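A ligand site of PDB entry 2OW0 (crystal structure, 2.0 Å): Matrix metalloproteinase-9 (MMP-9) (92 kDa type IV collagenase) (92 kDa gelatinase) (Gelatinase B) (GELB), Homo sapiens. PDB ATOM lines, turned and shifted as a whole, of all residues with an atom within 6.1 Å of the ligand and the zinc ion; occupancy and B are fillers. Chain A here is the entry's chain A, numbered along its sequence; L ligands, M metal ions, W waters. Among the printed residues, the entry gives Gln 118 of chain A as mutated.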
ATOM      1  N   PHE A   1     -27.511  22.371  -3.455  1.00  0.00           N
ATOM      2  CA  PHE A   1     -27.028  23.697  -2.965  1.00  0.00           C
ATOM      3  C   PHE A   1     -27.305  24.818  -3.967  1.00  0.00           C
ATOM      4  O   PHE A   1     -26.529  25.771  -4.061  1.00  0.00           O
ATOM      5  CB  PHE A   1     -25.530  23.640  -2.654  1.00  0.00           C
ATOM      6  CG  PHE A   1     -25.198  22.927  -1.377  1.00  0.00           C
ATOM      7  CD1 PHE A   1     -25.283  21.542  -1.297  1.00  0.00           C
ATOM      8  CD2 PHE A   1     -24.845  23.645  -0.244  1.00  0.00           C
ATOM      9  CE1 PHE A   1     -25.013  20.884  -0.095  1.00  0.00           C
ATOM     10  CE2 PHE A   1     -24.573  22.999   0.966  1.00  0.00           C
ATOM     11  CZ  PHE A   1     -24.658  21.612   1.036  1.00  0.00           C
ATOM     12  N   GLU A   2     -28.395  24.691  -4.712  1.00  0.00           N
ATOM     13  CA  GLU A   2     -28.774  25.696  -5.694  1.00  0.00           C
ATOM     14  C   GLU A   2     -30.104  26.297  -5.262  1.00  0.00           C
ATOM     15  O   GLU A   2     -31.095  25.583  -5.105  1.00  0.00           O
ATOM     16  CB  GLU A   2     -28.933  25.075  -7.085  1.00  0.00           C
ATOM     17  CG  GLU A   2     -27.755  25.290  -8.020  1.00  0.00           C
ATOM     18  N   GLY A  77     -11.436  16.055  -1.989  1.00  0.00           N
ATOM     19  CA  GLY A  77     -12.840  15.903  -2.323  1.00  0.00           C
ATOM     20  C   GLY A  77     -13.595  17.178  -2.018  1.00  0.00           C
ATOM     21  O   GLY A  77     -13.250  18.239  -2.531  1.00  0.00           O
ATOM     22  N   LEU A  78     -14.627  17.093  -1.185  1.00  0.00           N
ATOM     23  CA  LEU A  78     -15.385  18.296  -0.824  1.00  0.00           C
ATOM     24  C   LEU A  78     -14.501  19.179   0.052  1.00  0.00           C
ATOM     25  O   LEU A  78     -13.957  18.713   1.051  1.00  0.00           O
ATOM     26  CB  LEU A  78     -16.656  17.936  -0.056  1.00  0.00           C
ATOM     27  CG  LEU A  78     -17.805  17.336  -0.870  1.00  0.00           C
ATOM     28  CD1 LEU A  78     -18.950  16.921   0.058  1.00  0.00           C
ATOM     29  CD2 LEU A  78     -18.281  18.362  -1.880  1.00  0.00           C
ATOM     30  N   LEU A  79     -14.374  20.451  -0.330  1.00  0.00           N
ATOM     31  CA  LEU A  79     -13.571  21.414   0.413  1.00  0.00           C
ATOM     32  C   LEU A  79     -14.436  22.242   1.349  1.00  0.00           C
ATOM     33  O   LEU A  79     -13.990  22.649   2.417  1.00  0.00           O
ATOM     34  CB  LEU A  79     -12.860  22.361  -0.552  1.00  0.00           C
ATOM     35  CG  LEU A  79     -12.048  21.713  -1.660  1.00  0.00           C
ATOM     36  CD1 LEU A  79     -11.463  22.808  -2.528  1.00  0.00           C
ATOM     37  CD2 LEU A  79     -10.946  20.836  -1.073  1.00  0.00           C
ATOM     38  N   ALA A  80     -15.672  22.486   0.949  1.00  0.00           N
ATOM     39  CA  ALA A  80     -16.582  23.286   1.735  1.00  0.00           C
ATOM     40  C   ALA A  80     -17.877  23.481   0.955  1.00  0.00           C
ATOM     41  O   ALA A  80     -17.954  23.143  -0.225  1.00  0.00           O
ATOM     42  CB  ALA A  80     -15.947  24.647   2.020  1.00  0.00           C
ATOM     43  N   HIS A  81     -18.889  24.031   1.615  1.00  0.00           N
ATOM     44  CA  HIS A  81     -20.162  24.317   0.949  1.00  0.00           C
ATOM     45  C   HIS A  81     -20.894  25.401   1.705  1.00  0.00           C
ATOM     46  O   HIS A  81     -20.666  25.606   2.898  1.00  0.00           O
ATOM     47  CB  HIS A  81     -21.021  23.040   0.842  1.00  0.00           C
ATOM     48  CG  HIS A  81     -21.255  22.348   2.142  1.00  0.00           C
ATOM     49  ND1 HIS A  81     -21.399  20.980   2.226  1.00  0.00           N
ATOM     50  CD2 HIS A  81     -21.431  22.821   3.395  1.00  0.00           C
ATOM     51  CE1 HIS A  81     -21.654  20.642   3.482  1.00  0.00           C
ATOM     52  NE2 HIS A  81     -21.673  21.751   4.211  1.00  0.00           N
ATOM     53  N   ALA A  82     -21.767  26.106   0.989  1.00  0.00           N
ATOM     54  CA  ALA A  82     -22.539  27.206   1.555  1.00  0.00           C
ATOM     55  C   ALA A  82     -23.969  27.108   1.085  1.00  0.00           C
ATOM     56  O   ALA A  82     -24.219  26.898  -0.108  1.00  0.00           O
ATOM     57  CB  ALA A  82     -21.941  28.516   1.103  1.00  0.00           C
ATOM     58  N   LEU A 113      -9.543  32.444  -1.132  1.00  0.00           N
ATOM     59  CA  LEU A 113     -10.260  32.171  -2.374  1.00  0.00           C
ATOM     60  C   LEU A 113     -11.460  31.254  -2.193  1.00  0.00           C
ATOM     61  O   LEU A 113     -12.520  31.506  -2.791  1.00  0.00           O
ATOM     62  CB  LEU A 113      -9.311  31.565  -3.403  1.00  0.00           C
ATOM     63  CG  LEU A 113      -8.204  32.487  -3.896  1.00  0.00           C
ATOM     64  CD1 LEU A 113      -7.301  31.755  -4.881  1.00  0.00           C
ATOM     65  CD2 LEU A 113      -8.829  33.701  -4.585  1.00  0.00           C
ATOM     66  N   VAL A 114     -11.324  30.190  -1.413  1.00  0.00           N
ATOM     67  CA  VAL A 114     -12.442  29.281  -1.189  1.00  0.00           C
ATOM     68  C   VAL A 114     -13.558  30.020  -0.460  1.00  0.00           C
ATOM     69  O   VAL A 114     -14.727  29.858  -0.793  1.00  0.00           O
ATOM     70  CB  VAL A 114     -12.012  28.038  -0.380  1.00  0.00           C
ATOM     71  CG1 VAL A 114     -13.214  27.153  -0.093  1.00  0.00           C
ATOM     72  CG2 VAL A 114     -11.023  27.269  -1.170  1.00  0.00           C
ATOM     73  N   HIS A 117     -15.507  32.308  -2.799  1.00  0.00           N
ATOM     74  CA  HIS A 117     -16.320  31.435  -3.633  1.00  0.00           C
ATOM     75  C   HIS A 117     -17.570  31.043  -2.837  1.00  0.00           C
ATOM     76  O   HIS A 117     -18.687  31.195  -3.325  1.00  0.00           O
ATOM     77  CB  HIS A 117     -15.547  30.164  -4.000  1.00  0.00           C
ATOM     78  CG  HIS A 117     -16.324  29.185  -4.840  1.00  0.00           C
ATOM     79  ND1 HIS A 117     -16.230  29.162  -6.222  1.00  0.00           N
ATOM     80  CD2 HIS A 117     -17.190  28.208  -4.510  1.00  0.00           C
ATOM     81  CE1 HIS A 117     -17.016  28.206  -6.690  1.00  0.00           C
ATOM     82  NE2 HIS A 117     -17.604  27.606  -5.670  1.00  0.00           N
ATOM     83  N   GLN A 118     -17.365  30.540  -1.630  1.00  0.00           N
ATOM     84  CA  GLN A 118     -18.491  30.123  -0.793  1.00  0.00           C
ATOM     85  C   GLN A 118     -19.435  31.298  -0.505  1.00  0.00           C
ATOM     86  O   GLN A 118     -20.662  31.136  -0.544  1.00  0.00           O
ATOM     87  CB  GLN A 118     -18.002  29.514   0.530  1.00  0.00           C
ATOM     88  CG  GLN A 118     -17.182  28.233   0.392  1.00  0.00           C
ATOM     89  CD  GLN A 118     -17.907  27.184  -0.411  1.00  0.00           C
ATOM     90  OE1 GLN A 118     -19.091  26.928  -0.173  1.00  0.00           O
ATOM     91  NE2 GLN A 118     -17.218  26.560  -1.356  1.00  0.00           N
ATOM     92  N   HIS A 121     -21.877  31.751  -3.147  1.00  0.00           N
ATOM     93  CA  HIS A 121     -23.015  30.846  -3.037  1.00  0.00           C
ATOM     94  C   HIS A 121     -23.981  31.361  -1.959  1.00  0.00           C
ATOM     95  O   HIS A 121     -25.207  31.319  -2.135  1.00  0.00           O
ATOM     96  CB  HIS A 121     -22.557  29.427  -2.661  1.00  0.00           C
ATOM     97  CG  HIS A 121     -21.939  28.660  -3.783  1.00  0.00           C
ATOM     98  ND1 HIS A 121     -22.557  28.501  -5.003  1.00  0.00           N
ATOM     99  CD2 HIS A 121     -20.769  27.970  -3.866  1.00  0.00           C
ATOM    100  CE1 HIS A 121     -21.810  27.756  -5.787  1.00  0.00           C
ATOM    101  NE2 HIS A 121     -20.717  27.412  -5.128  1.00  0.00           N
ATOM    102  N   HIS A 127     -22.766  28.367  -9.932  1.00  0.00           N
ATOM    103  CA  HIS A 127     -21.502  28.156 -10.612  1.00  0.00           C
ATOM    104  C   HIS A 127     -21.439  28.795 -11.990  1.00  0.00           C
ATOM    105  O   HIS A 127     -22.427  28.790 -12.726  1.00  0.00           O
ATOM    106  CB  HIS A 127     -21.225  26.656 -10.727  1.00  0.00           C
ATOM    107  CG  HIS A 127     -20.687  26.052  -9.474  1.00  0.00           C
ATOM    108  ND1 HIS A 127     -20.905  24.733  -9.137  1.00  0.00           N
ATOM    109  CD2 HIS A 127     -19.914  26.574  -8.497  1.00  0.00           C
ATOM    110  CE1 HIS A 127     -20.290  24.477  -7.994  1.00  0.00           C
ATOM    111  NE2 HIS A 127     -19.682  25.574  -7.584  1.00  0.00           N
ATOM    112  N   ALA A 133     -13.420  32.590 -13.821  1.00  0.00           N
ATOM    113  CA  ALA A 133     -14.308  33.183 -12.827  1.00  0.00           C
ATOM    114  C   ALA A 133     -14.157  32.573 -11.436  1.00  0.00           C
ATOM    115  O   ALA A 133     -13.931  31.379 -11.300  1.00  0.00           O
ATOM    116  CB  ALA A 133     -15.743  33.072 -13.263  1.00  0.00           C
ATOM    117  N   LEU A 134     -14.327  33.401 -10.409  1.00  0.00           N
ATOM    118  CA  LEU A 134     -14.252  32.891  -9.042  1.00  0.00           C
ATOM    119  C   LEU A 134     -15.297  31.783  -8.815  1.00  0.00           C
ATOM    120  O   LEU A 134     -15.031  30.795  -8.117  1.00  0.00           O
ATOM    121  CB  LEU A 134     -14.503  34.037  -8.065  1.00  0.00           C
ATOM    122  CG  LEU A 134     -14.651  33.673  -6.584  1.00  0.00           C
ATOM    123  CD1 LEU A 134     -13.393  32.984  -6.060  1.00  0.00           C
ATOM    124  CD2 LEU A 134     -14.892  34.943  -5.816  1.00  0.00           C
ATOM    125  N   MET A 135     -16.482  31.953  -9.411  1.00  0.00           N
ATOM    126  CA  MET A 135     -17.543  30.967  -9.230  1.00  0.00           C
ATOM    127  C   MET A 135     -17.406  29.732 -10.122  1.00  0.00           C
ATOM    128  O   MET A 135     -18.363  28.986 -10.294  1.00  0.00           O
ATOM    129  CB  MET A 135     -18.910  31.592  -9.429  1.00  0.00           C
ATOM    130  CG  MET A 135     -19.246  32.665  -8.399  1.00  0.00           C
ATOM    131  SD  MET A 135     -18.940  32.185  -6.671  1.00  0.00           S
ATOM    132  CE  MET A 135     -20.089  30.838  -6.408  1.00  0.00           C
ATOM    133  N   TYR A 136     -16.222  29.534 -10.685  1.00  0.00           N
ATOM    134  CA  TYR A 136     -15.976  28.350 -11.491  1.00  0.00           C
ATOM    135  C   TYR A 136     -16.057  27.167 -10.492  1.00  0.00           C
ATOM    136  O   TYR A 136     -15.595  27.286  -9.362  1.00  0.00           O
ATOM    137  CB  TYR A 136     -14.601  28.433 -12.135  1.00  0.00           C
ATOM    138  CG  TYR A 136     -14.352  27.406 -13.209  1.00  0.00           C
ATOM    139  CD1 TYR A 136     -15.158  27.356 -14.347  1.00  0.00           C
ATOM    140  CD2 TYR A 136     -13.280  26.513 -13.121  1.00  0.00           C
ATOM    141  CE1 TYR A 136     -14.909  26.434 -15.371  1.00  0.00           C
ATOM    142  CE2 TYR A 136     -13.022  25.590 -14.134  1.00  0.00           C
ATOM    143  CZ  TYR A 136     -13.845  25.559 -15.256  1.00  0.00           C
ATOM    144  OH  TYR A 136     -13.563  24.652 -16.262  1.00  0.00           O
ATOM    145  N   PRO A 137     -16.634  26.029 -10.903  1.00  0.00           N
ATOM    146  CA  PRO A 137     -16.773  24.859 -10.021  1.00  0.00           C
ATOM    147  C   PRO A 137     -15.496  24.102  -9.655  1.00  0.00           C
ATOM    148  O   PRO A 137     -15.511  23.211  -8.795  1.00  0.00           O
ATOM    149  CB  PRO A 137     -17.774  23.970 -10.767  1.00  0.00           C
ATOM    150  CG  PRO A 137     -17.500  24.282 -12.180  1.00  0.00           C
ATOM    151  CD  PRO A 137     -17.278  25.777 -12.206  1.00  0.00           C
ATOM    152  N   MET A 138     -14.396  24.494 -10.283  1.00  0.00           N
ATOM    153  CA  MET A 138     -13.105  23.865 -10.057  1.00  0.00           C
ATOM    154  C   MET A 138     -12.112  24.789  -9.358  1.00  0.00           C
ATOM    155  O   MET A 138     -11.881  25.918  -9.788  1.00  0.00           O
ATOM    156  CB  MET A 138     -12.530  23.426 -11.392  1.00  0.00           C
ATOM    157  CG  MET A 138     -12.476  21.942 -11.623  1.00  0.00           C
ATOM    158  SD  MET A 138     -10.976  21.256 -10.915  1.00  0.00           S
ATOM    159  CE  MET A 138      -9.705  22.282 -11.678  1.00  0.00           C
ATOM    160  N   TYR A 139     -11.505  24.311  -8.282  1.00  0.00           N
ATOM    161  CA  TYR A 139     -10.537  25.138  -7.575  1.00  0.00           C
ATOM    162  C   TYR A 139      -9.171  25.118  -8.270  1.00  0.00           C
ATOM    163  O   TYR A 139      -8.714  24.060  -8.684  1.00  0.00           O
ATOM    164  CB  TYR A 139     -10.331  24.635  -6.153  1.00  0.00           C
ATOM    165  CG  TYR A 139      -9.210  25.370  -5.441  1.00  0.00           C
ATOM    166  CD1 TYR A 139      -9.459  26.548  -4.726  1.00  0.00           C
ATOM    167  CD2 TYR A 139      -7.889  24.917  -5.505  1.00  0.00           C
ATOM    168  CE1 TYR A 139      -8.417  27.264  -4.105  1.00  0.00           C
ATOM    169  CE2 TYR A 139      -6.840  25.622  -4.882  1.00  0.00           C
ATOM    170  CZ  TYR A 139      -7.119  26.793  -4.187  1.00  0.00           C
ATOM    171  OH  TYR A 139      -6.113  27.531  -3.562  1.00  0.00           O
ATOM    172  N   ARG A 140      -8.540  26.277  -8.372  1.00  0.00           N
ATOM    173  CA  ARG A 140      -7.207  26.370  -8.969  1.00  0.00           C
ATOM    174  C   ARG A 140      -6.611  27.699  -8.474  1.00  0.00           C
ATOM    175  O   ARG A 140      -7.174  28.755  -8.698  1.00  0.00           O
ATOM    176  CB  ARG A 140      -7.289  26.332 -10.508  1.00  0.00           C
ATOM    177  CG  ARG A 140      -5.956  26.100 -11.201  1.00  0.00           C
ATOM    178  N   THR A 142      -4.487  31.002  -8.388  1.00  0.00           N
ATOM    179  CA  THR A 142      -3.914  31.937  -9.335  1.00  0.00           C
ATOM    180  C   THR A 142      -3.820  33.286  -8.621  1.00  0.00           C
ATOM    181  O   THR A 142      -4.543  33.535  -7.650  1.00  0.00           O
ATOM    182  CB  THR A 142      -4.775  32.125 -10.576  1.00  0.00           C
ATOM    183  OG1 THR A 142      -6.026  32.725 -10.202  1.00  0.00           O
ATOM    184  CG2 THR A 142      -5.019  30.768 -11.265  1.00  0.00           C
HETATM  185  C1  LIG L   1     -21.594  22.462  -4.910  1.00  0.00           C
HETATM  186  C2  LIG L   1     -22.137  23.748  -4.853  1.00  0.00           C
HETATM  187  C3  LIG L   1     -23.050  24.162  -5.817  1.00  0.00           C
HETATM  188  C4  LIG L   1     -23.429  23.293  -6.838  1.00  0.00           C
HETATM  189  C5  LIG L   1     -22.897  22.011  -6.896  1.00  0.00           C
HETATM  190  C6  LIG L   1     -21.984  21.596  -5.932  1.00  0.00           C
HETATM  191  N1  LIG L   1     -21.337  20.447  -5.747  1.00  0.00           N
HETATM  192  C7  LIG L   1     -20.565  20.548  -4.662  1.00  0.00           C
HETATM  193  C8  LIG L   1     -20.695  21.764  -4.123  1.00  0.00           C
HETATM  194  C9  LIG L   1     -19.960  22.275  -2.880  1.00  0.00           C
HETATM  195  C10 LIG L   1     -18.578  22.871  -3.211  1.00  0.00           C
HETATM  196  C11 LIG L   1     -18.767  24.182  -3.983  1.00  0.00           C
HETATM  197  O1  LIG L   1     -18.606  24.147  -5.226  1.00  0.00           O
HETATM  198  O2  LIG L   1     -19.084  25.189  -3.317  1.00  0.00           O
HETATM  199  N2  LIG L   1     -17.822  21.906  -4.021  1.00  0.00           N
HETATM  200  S1  LIG L   1     -16.225  21.925  -3.671  1.00  0.00           S
HETATM  201  O3  LIG L   1     -15.592  20.707  -4.280  1.00  0.00           O
HETATM  202  O4  LIG L   1     -16.033  21.852  -2.175  1.00  0.00           O
HETATM  203  C12 LIG L   1     -15.462  23.367  -4.297  1.00  0.00           C
HETATM  204  C13 LIG L   1     -15.532  24.561  -3.577  1.00  0.00           C
HETATM  205  C14 LIG L   1     -14.946  25.719  -4.070  1.00  0.00           C
HETATM  206  C15 LIG L   1     -14.810  23.361  -5.525  1.00  0.00           C
HETATM  207  C16 LIG L   1     -14.222  24.528  -6.020  1.00  0.00           C
HETATM  208  C17 LIG L   1     -14.294  25.712  -5.298  1.00  0.00           C
HETATM  209  C18 LIG L   1     -13.696  26.877  -5.792  1.00  0.00           C
HETATM  210  C19 LIG L   1     -13.037  27.762  -4.946  1.00  0.00           C
HETATM  211  C20 LIG L   1     -12.298  28.820  -5.473  1.00  0.00           C
HETATM  212  C21 LIG L   1     -12.203  29.008  -6.847  1.00  0.00           C
HETATM  213  I1  LIG L   1     -10.998  30.562  -7.590  1.00  0.00           I
HETATM  214  C22 LIG L   1     -12.870  28.135  -7.696  1.00  0.00           C
HETATM  215  C23 LIG L   1     -13.618  27.080  -7.170  1.00  0.00           C
HETATM  216 ZN    ZN M   1     -19.147  26.152  -5.688  1.00  0.00          ZN
HETATM  217  O   HOH W   1      -7.887  31.186  -9.051  1.00  0.00           O
HETATM  218  O   HOH W   2     -17.862  22.199  -7.192  1.00  0.00           O
HETATM  219  O   HOH W   3     -21.528  25.560  -1.780  1.00  0.00           O
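The backbone NH of Leu 79 lies within hydrogen-bond range of an oxygen (O4) of the ligand, at 2.8 Å.
The backbone NH of Ala 80 is in hydrogen-bond range of an oxygen (O4) of the ligand, 3.2 Å away.
An oxygen (O2) of the ligand lies close to the side-chain amide nitrogen of Gln 118.
O of Leu 134 sits at hydrogen-bond distance from ND1 of His 117 (2.8 Å).
The side-chain amide oxygen of Gln 118 lies close to the backbone NH of His 81, at 3.4 Å.
The side-chain amide oxygen (OE1) of Gln 118 is in hydrogen-bond range of the backbone NH (N) of Ala 82.
Gly 77 touches the ligand (O to O3, 3.8 Å).
Leu 78 touches the ligand.
His 81 touches the ligand.
Leu 113 touches the ligand (O to C20, 3.8 Å).
Leu 134 touches the ligand (O to C22, 3.5 Å).
Tyr 136 touches the ligand.
Pro 137 touches the ligand (O to C16, 3.3 Å).
Met 138 touches the ligand.
N of Tyr 139 touches C16 of the ligand, 3.5 Å away.
Hydrophobic or aromatic side chains within 4 Å of the ligand: Leu 79, His 81, His 117, His 121, His 127, Leu 134 and Tyr 139.
15 residues have an atom within 4 Å of the ligand: Gly 77, Leu 78, Leu 79, Ala 80, His 81, Leu 113, His 117, Gln 118, His 121, His 127, Leu 134, Tyr 136, Pro 137, Met 138 and Tyr 139.
Along chain A the residues within 4 Å of the ligand span positions 77 to 139.
The nearest printed residue that does not touch the ligand is Phe 1 (4.04 Å).
Three residues have an atom within 4 Å of the zinc ion: His 117, His 121 and His 127.
The zinc ion is bound by a ring nitrogen (NE2) of His 127 (2.1 Å), a ring nitrogen (NE2) of His 121 (2.1 Å), a ring nitrogen (NE2) of His 117 (2.1 Å), an oxygen (O1) of the ligand (2.1 Å) and an oxygen (O2) of the ligand (2.6 Å).
The zinc ion has five donor atoms within binding distance.
Water W2 bridges O of Pro 137 (3.0 Å) and N2 of the ligand (3.2 Å).
Water W3 bridges N of Ala 82 and OE1 of Gln 118.
Water W1 bridges O of Arg 140 (2.6 Å) and OG1 of Thr 142 (2.7 Å).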
